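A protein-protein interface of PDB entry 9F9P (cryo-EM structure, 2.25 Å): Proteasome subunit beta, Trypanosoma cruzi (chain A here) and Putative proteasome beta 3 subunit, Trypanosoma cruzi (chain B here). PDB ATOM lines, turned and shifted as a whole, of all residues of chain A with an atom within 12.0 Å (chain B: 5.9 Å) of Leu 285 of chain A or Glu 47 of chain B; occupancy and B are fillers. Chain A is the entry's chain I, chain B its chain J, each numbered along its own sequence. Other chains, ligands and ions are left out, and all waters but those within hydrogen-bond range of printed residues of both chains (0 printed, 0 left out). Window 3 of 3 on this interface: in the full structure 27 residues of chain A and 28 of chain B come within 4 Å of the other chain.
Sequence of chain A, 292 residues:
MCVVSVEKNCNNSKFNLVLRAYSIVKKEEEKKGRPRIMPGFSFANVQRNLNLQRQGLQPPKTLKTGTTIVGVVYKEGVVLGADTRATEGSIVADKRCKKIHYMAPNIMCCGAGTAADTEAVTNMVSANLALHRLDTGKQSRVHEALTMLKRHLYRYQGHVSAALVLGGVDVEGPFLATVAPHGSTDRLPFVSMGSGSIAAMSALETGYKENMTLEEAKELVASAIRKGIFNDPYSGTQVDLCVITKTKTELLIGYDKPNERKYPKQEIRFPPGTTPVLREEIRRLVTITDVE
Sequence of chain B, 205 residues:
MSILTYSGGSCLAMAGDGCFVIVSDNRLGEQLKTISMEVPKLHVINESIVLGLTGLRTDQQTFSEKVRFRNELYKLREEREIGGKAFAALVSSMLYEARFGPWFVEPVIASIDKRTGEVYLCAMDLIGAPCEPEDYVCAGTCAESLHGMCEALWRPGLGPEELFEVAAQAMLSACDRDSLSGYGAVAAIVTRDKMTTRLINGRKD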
ATOM      1  N   GLU A 281     -22.206  21.415 -13.581  1.00  0.00           N
ATOM      2  CA  GLU A 281     -22.384  20.101 -14.191  1.00  0.00           C
ATOM      3  C   GLU A 281     -22.223  19.015 -13.122  1.00  0.00           C
ATOM      4  O   GLU A 281     -21.426  19.173 -12.194  1.00  0.00           O
ATOM      5  CB  GLU A 281     -21.377  19.859 -15.316  1.00  0.00           C
ATOM      6  CG  GLU A 281     -21.502  20.826 -16.479  1.00  0.00           C
ATOM      7  CD  GLU A 281     -20.454  20.622 -17.569  1.00  0.00           C
ATOM      8  OE1 GLU A 281     -19.236  20.637 -17.238  1.00  0.00           O
ATOM      9  OE2 GLU A 281     -20.851  20.448 -18.750  1.00  0.00           O
ATOM     10  N   ILE A 282     -22.982  17.914 -13.287  1.00  0.00           N
ATOM     11  CA  ILE A 282     -22.966  16.772 -12.375  1.00  0.00           C
ATOM     12  C   ILE A 282     -22.667  15.491 -13.160  1.00  0.00           C
ATOM     13  O   ILE A 282     -22.940  15.405 -14.359  1.00  0.00           O
ATOM     14  CB  ILE A 282     -24.281  16.679 -11.563  1.00  0.00           C
ATOM     15  CG1 ILE A 282     -24.671  18.041 -10.972  1.00  0.00           C
ATOM     16  CG2 ILE A 282     -24.194  15.594 -10.495  1.00  0.00           C
ATOM     17  CD1 ILE A 282     -25.368  18.001  -9.620  1.00  0.00           C
ATOM     18  N   ARG A 283     -22.063  14.515 -12.468  1.00  0.00           N
ATOM     19  CA  ARG A 283     -21.741  13.220 -13.050  1.00  0.00           C
ATOM     20  C   ARG A 283     -21.784  12.143 -11.960  1.00  0.00           C
ATOM     21  O   ARG A 283     -21.181  12.302 -10.900  1.00  0.00           O
ATOM     22  CB  ARG A 283     -20.394  13.318 -13.776  1.00  0.00           C
ATOM     23  CG  ARG A 283     -19.760  11.979 -14.133  1.00  0.00           C
ATOM     24  CD  ARG A 283     -18.741  12.066 -15.254  1.00  0.00           C
ATOM     25  NE  ARG A 283     -17.850  13.217 -15.141  1.00  0.00           N
ATOM     26  CZ  ARG A 283     -16.523  13.157 -15.049  1.00  0.00           C
ATOM     27  NH1 ARG A 283     -15.902  11.990 -15.040  1.00  0.00           N
ATOM     28  NH2 ARG A 283     -15.821  14.274 -14.963  1.00  0.00           N
ATOM     29  N   ARG A 284     -22.514  11.048 -12.240  1.00  0.00           N
ATOM     30  CA  ARG A 284     -22.599   9.881 -11.369  1.00  0.00           C
ATOM     31  C   ARG A 284     -21.531   8.860 -11.767  1.00  0.00           C
ATOM     32  O   ARG A 284     -21.195   8.746 -12.946  1.00  0.00           O
ATOM     33  CB  ARG A 284     -23.984   9.232 -11.471  1.00  0.00           C
ATOM     34  CG  ARG A 284     -25.143  10.171 -11.168  1.00  0.00           C
ATOM     35  CD  ARG A 284     -25.339  10.422  -9.685  1.00  0.00           C
ATOM     36  NE  ARG A 284     -26.054  11.672  -9.450  1.00  0.00           N
ATOM     37  CZ  ARG A 284     -26.534  12.066  -8.275  1.00  0.00           C
ATOM     38  NH1 ARG A 284     -26.495  11.254  -7.233  1.00  0.00           N
ATOM     39  NH2 ARG A 284     -27.078  13.265  -8.152  1.00  0.00           N
ATOM     40  N   LEU A 285     -21.041   8.091 -10.778  1.00  0.00           N
ATOM     41  CA  LEU A 285     -19.821   7.302 -10.917  1.00  0.00           C
ATOM     42  C   LEU A 285     -20.146   5.797 -10.932  1.00  0.00           C
ATOM     43  O   LEU A 285     -20.794   5.321  -9.973  1.00  0.00           O
ATOM     44  CB  LEU A 285     -18.860   7.676  -9.775  1.00  0.00           C
ATOM     45  CG  LEU A 285     -18.389   9.139  -9.727  1.00  0.00           C
ATOM     46  CD1 LEU A 285     -17.384   9.364  -8.604  1.00  0.00           C
ATOM     47  CD2 LEU A 285     -17.782   9.607 -11.047  1.00  0.00           C
ATOM     48  N   VAL B  44      -8.718  15.859 -15.265  1.00  0.00           N
ATOM     49  CA  VAL B  44      -9.272  14.659 -14.686  1.00  0.00           C
ATOM     50  C   VAL B  44      -8.573  13.392 -15.212  1.00  0.00           C
ATOM     51  O   VAL B  44      -8.648  13.099 -16.394  1.00  0.00           O
ATOM     52  CB  VAL B  44     -10.791  14.584 -14.922  1.00  0.00           C
ATOM     53  CG1 VAL B  44     -11.390  13.310 -14.338  1.00  0.00           C
ATOM     54  CG2 VAL B  44     -11.508  15.781 -14.304  1.00  0.00           C
ATOM     55  N   ILE B  45      -7.967  12.606 -14.315  1.00  0.00           N
ATOM     56  CA  ILE B  45      -7.189  11.421 -14.668  1.00  0.00           C
ATOM     57  C   ILE B  45      -8.054  10.155 -14.688  1.00  0.00           C
ATOM     58  O   ILE B  45      -7.928   9.331 -15.575  1.00  0.00           O
ATOM     59  CB  ILE B  45      -5.996  11.276 -13.708  1.00  0.00           C
ATOM     60  CG1 ILE B  45      -5.066  12.496 -13.762  1.00  0.00           C
ATOM     61  CG2 ILE B  45      -5.239   9.991 -13.976  1.00  0.00           C
ATOM     62  CD1 ILE B  45      -4.368  12.732 -15.112  1.00  0.00           C
ATOM     63  N   ASN B  46      -8.952  10.019 -13.722  1.00  0.00           N
ATOM     64  CA  ASN B  46      -9.998   9.003 -13.688  1.00  0.00           C
ATOM     65  C   ASN B  46     -10.984   9.453 -12.633  1.00  0.00           C
ATOM     66  O   ASN B  46     -10.799  10.509 -12.061  1.00  0.00           O
ATOM     67  CB  ASN B  46      -9.459   7.593 -13.388  1.00  0.00           C
ATOM     68  CG  ASN B  46      -8.674   7.455 -12.104  1.00  0.00           C
ATOM     69  OD1 ASN B  46      -9.017   8.030 -11.081  1.00  0.00           O
ATOM     70  ND2 ASN B  46      -7.570   6.737 -12.151  1.00  0.00           N
ATOM     71  N   GLU B  47     -11.959   8.635 -12.291  1.00  0.00           N
ATOM     72  CA  GLU B  47     -13.041   9.068 -11.419  1.00  0.00           C
ATOM     73  C   GLU B  47     -12.547   9.461 -10.032  1.00  0.00           C
ATOM     74  O   GLU B  47     -13.232  10.174  -9.312  1.00  0.00           O
ATOM     75  CB  GLU B  47     -14.074   7.950 -11.251  1.00  0.00           C
ATOM     76  CG  GLU B  47     -14.874   7.653 -12.519  1.00  0.00           C
ATOM     77  CD  GLU B  47     -15.926   6.543 -12.394  1.00  0.00           C
ATOM     78  OE1 GLU B  47     -15.952   5.843 -11.333  1.00  0.00           O
ATOM     79  OE2 GLU B  47     -16.741   6.378 -13.350  1.00  0.00           O
ATOM     80  N   SER B  48     -11.402   8.953  -9.628  1.00  0.00           N
ATOM     81  CA  SER B  48     -10.913   9.151  -8.275  1.00  0.00           C
ATOM     82  C   SER B  48      -9.816  10.210  -8.164  1.00  0.00           C
ATOM     83  O   SER B  48      -9.407  10.452  -7.052  1.00  0.00           O
ATOM     84  CB  SER B  48     -10.378   7.806  -7.723  1.00  0.00           C
ATOM     85  OG  SER B  48     -11.428   6.907  -7.349  1.00  0.00           O
ATOM     86  N   ILE B  49      -9.275  10.752  -9.253  1.00  0.00           N
ATOM     87  CA  ILE B  49      -8.063  11.554  -9.219  1.00  0.00           C
ATOM     88  C   ILE B  49      -8.155  12.767 -10.138  1.00  0.00           C
ATOM     89  O   ILE B  49      -8.417  12.602 -11.313  1.00  0.00           O
ATOM     90  CB  ILE B  49      -6.833  10.757  -9.704  1.00  0.00           C
ATOM     91  CG1 ILE B  49      -6.616   9.474  -8.936  1.00  0.00           C
ATOM     92  CG2 ILE B  49      -5.551  11.588  -9.711  1.00  0.00           C
ATOM     93  CD1 ILE B  49      -5.396   8.748  -9.424  1.00  0.00           C
ATOM     94  N   ILE B 112      -9.269  10.176  -3.880  1.00  0.00           N
ATOM     95  CA  ILE B 112     -10.061   9.502  -2.869  1.00  0.00           C
ATOM     96  C   ILE B 112     -10.087   8.014  -3.203  1.00  0.00           C
ATOM     97  O   ILE B 112     -10.417   7.651  -4.327  1.00  0.00           O
ATOM     98  CB  ILE B 112     -11.468  10.131  -2.861  1.00  0.00           C
ATOM     99  CG1 ILE B 112     -12.350   9.604  -1.745  1.00  0.00           C
ATOM    100  CG2 ILE B 112     -12.177   9.974  -4.201  1.00  0.00           C
ATOM    101  CD1 ILE B 112     -13.606  10.436  -1.606  1.00  0.00           C
ATOM    102  N   VAL B 190     -15.446  16.160  -5.358  1.00  0.00           N
ATOM    103  CA  VAL B 190     -15.422  14.725  -5.591  1.00  0.00           C
ATOM    104  C   VAL B 190     -15.794  13.961  -4.333  1.00  0.00           C
ATOM    105  O   VAL B 190     -15.241  14.214  -3.267  1.00  0.00           O
ATOM    106  CB  VAL B 190     -14.037  14.318  -6.108  1.00  0.00           C
ATOM    107  CG1 VAL B 190     -13.944  12.829  -6.376  1.00  0.00           C
ATOM    108  CG2 VAL B 190     -13.658  15.120  -7.355  1.00  0.00           C
ATOM    109  N   THR B 191     -16.779  13.067  -4.448  1.00  0.00           N
ATOM    110  CA  THR B 191     -17.107  12.116  -3.376  1.00  0.00           C
ATOM    111  C   THR B 191     -16.911  10.710  -3.932  1.00  0.00           C
ATOM    112  O   THR B 191     -16.572  10.569  -5.117  1.00  0.00           O
ATOM    113  CB  THR B 191     -18.531  12.306  -2.842  1.00  0.00           C
ATOM    114  OG1 THR B 191     -19.455  11.960  -3.867  1.00  0.00           O
ATOM    115  CG2 THR B 191     -18.848  13.729  -2.437  1.00  0.00           C
ATOM    116  N   ARG B 192     -17.176   9.682  -3.115  1.00  0.00           N
ATOM    117  CA  ARG B 192     -17.165   8.301  -3.604  1.00  0.00           C
ATOM    118  C   ARG B 192     -18.194   8.110  -4.722  1.00  0.00           C
ATOM    119  O   ARG B 192     -17.912   7.432  -5.704  1.00  0.00           O
ATOM    120  CB  ARG B 192     -17.500   7.314  -2.486  1.00  0.00           C
ATOM    121  CG  ARG B 192     -16.630   7.431  -1.247  1.00  0.00           C
ATOM    122  CD  ARG B 192     -17.113   6.506  -0.141  1.00  0.00           C
ATOM    123  NE  ARG B 192     -17.105   7.219   1.131  1.00  0.00           N
ATOM    124  CZ  ARG B 192     -16.920   6.657   2.320  1.00  0.00           C
ATOM    125  NH1 ARG B 192     -16.894   7.414   3.405  1.00  0.00           N
ATOM    126  NH2 ARG B 192     -16.734   5.350   2.415  1.00  0.00           N
ATOM    127  N   ASP B 193     -19.352   8.774  -4.575  1.00  0.00           N
ATOM    128  CA  ASP B 193     -20.547   8.539  -5.370  1.00  0.00           C
ATOM    129  C   ASP B 193     -20.620   9.428  -6.611  1.00  0.00           C
ATOM    130  O   ASP B 193     -21.144   8.990  -7.631  1.00  0.00           O
ATOM    131  CB  ASP B 193     -21.820   8.799  -4.550  1.00  0.00           C
ATOM    132  CG  ASP B 193     -21.999   7.911  -3.322  1.00  0.00           C
ATOM    133  OD1 ASP B 193     -21.188   6.970  -3.138  1.00  0.00           O
ATOM    134  OD2 ASP B 193     -22.952   8.169  -2.548  1.00  0.00           O
ATOM    135  N   LYS B 194     -20.192  10.696  -6.525  1.00  0.00           N
ATOM    136  CA  LYS B 194     -20.345  11.574  -7.674  1.00  0.00           C
ATOM    137  C   LYS B 194     -19.193  12.572  -7.806  1.00  0.00           C
ATOM    138  O   LYS B 194     -18.368  12.723  -6.905  1.00  0.00           O
ATOM    139  CB  LYS B 194     -21.704  12.278  -7.618  1.00  0.00           C
ATOM    140  CG  LYS B 194     -21.886  13.346  -6.557  1.00  0.00           C
ATOM    141  CD  LYS B 194     -23.355  13.613  -6.286  1.00  0.00           C
ATOM    142  CE  LYS B 194     -23.626  14.697  -5.260  1.00  0.00           C
ATOM    143  NZ  LYS B 194     -23.987  15.982  -5.910  1.00  0.00           N
ATOM    144  N   MET B 195     -19.151  13.219  -8.977  1.00  0.00           N
ATOM    145  CA  MET B 195     -18.261  14.336  -9.221  1.00  0.00           C
ATOM    146  C   MET B 195     -19.044  15.519  -9.789  1.00  0.00           C
ATOM    147  O   MET B 195     -19.588  15.459 -10.886  1.00  0.00           O
ATOM    148  CB  MET B 195     -17.133  13.982 -10.191  1.00  0.00           C
ATOM    149  CG  MET B 195     -16.346  15.251 -10.593  1.00  0.00           C
ATOM    150  SD  MET B 195     -14.853  15.046 -11.574  1.00  0.00           S
ATOM    151  CE  MET B 195     -14.168  13.506 -10.944  1.00  0.00           C
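Glu 281 of chain A touches none of the printed residues of chain B. Of the printed residues of chain B, Ile 282 of chain A touches Met 195 (3.8 Å). Of the printed residues of chain B, Arg 283 of chain A touches Lys 194 (3.3 Å) and Met 195 (2.9 Å). Leu 285 of chain A touches just these residues of chain B: Glu 47 (3.8 Å), Thr 191 (3.8 Å), Arg 192 (3.5 Å), Asp 193 (3.3 Å) and Lys 194 (3.7 Å). Ile 45 of chain B touches none of the printed residues of chain A. Asn 46 of chain B touches none of the printed residues of chain A. Glu 47 of chain B touches one residue of chain A. No residue of chain A comes within 4 Å of Ser 48 of chain B. No residue of chain A comes within 4 Å of Ile 112 of chain B. No residue of chain A comes within 4 Å of Val 190 of chain B. Of chain A, only Leu 285 (3.8 Å) comes within 4 Å of Thr 191 of chain B. Printed residues of chain A within 4 Å of Arg 192 of chain B: Leu 285. Of the printed residues of chain A, Asp 193 of chain B touches Leu 285 (3.3 Å). Of the printed residues of chain A, Lys 194 of chain B touches Arg 283 and Leu 285. The nearest printed residue of chain B that does not touch Ile 282 of chain A is Lys 194 of chain B (4.4 Å).
Hydrophobic or aromatic side chains of chain A within 4 Å of the printed part of chain B: Leu 285. Of the 13 printed residues of chain B, 6 touch a printed residue of chain A. Printed residues of chain B that touch a printed residue of chain A: Glu 47, Thr 191, Arg 192, Asp 193, Lys 194 and Met 195. Hydrophobic or aromatic side chains of chain B that line the printed part of chain A: Met 195. Among the printed residues, no Asp or Glu carboxylate lies within 4 Å of a Lys or Arg side-chain nitrogen of the other chain.
Met 195 of chain B touches Ile 282 of chain A (O to C, 3.8 Å). O of Arg 283 of chain A touches CB of Lys 194 of chain B (3.3 Å). Leu 285 of chain A touches Glu 47 of chain B. Thr 191 of chain B touches Leu 285 of chain A (O to CD1, 3.8 Å). O of Arg 192 of chain B touches CD1 of Leu 285 of chain A (3.5 Å). CG of Leu 285 of chain A touches CA of Lys 194 of chain B (3.7 Å).
The backbone NH of Asp 193 of chain B sits close to the side-chain hydroxyl of Thr 191 of chain B, at 3.3 Å. N of Lys 194 of chain B lies within hydrogen-bond range of OG1 of Thr 191 of chain B.
N of Leu 285 of chain A is in hydrogen-bond range of O of Asp 193 of chain B (3.3 Å). O of Arg 283 of chain A sits at hydrogen-bond distance from N of Met 195 of chain B (2.9 Å).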
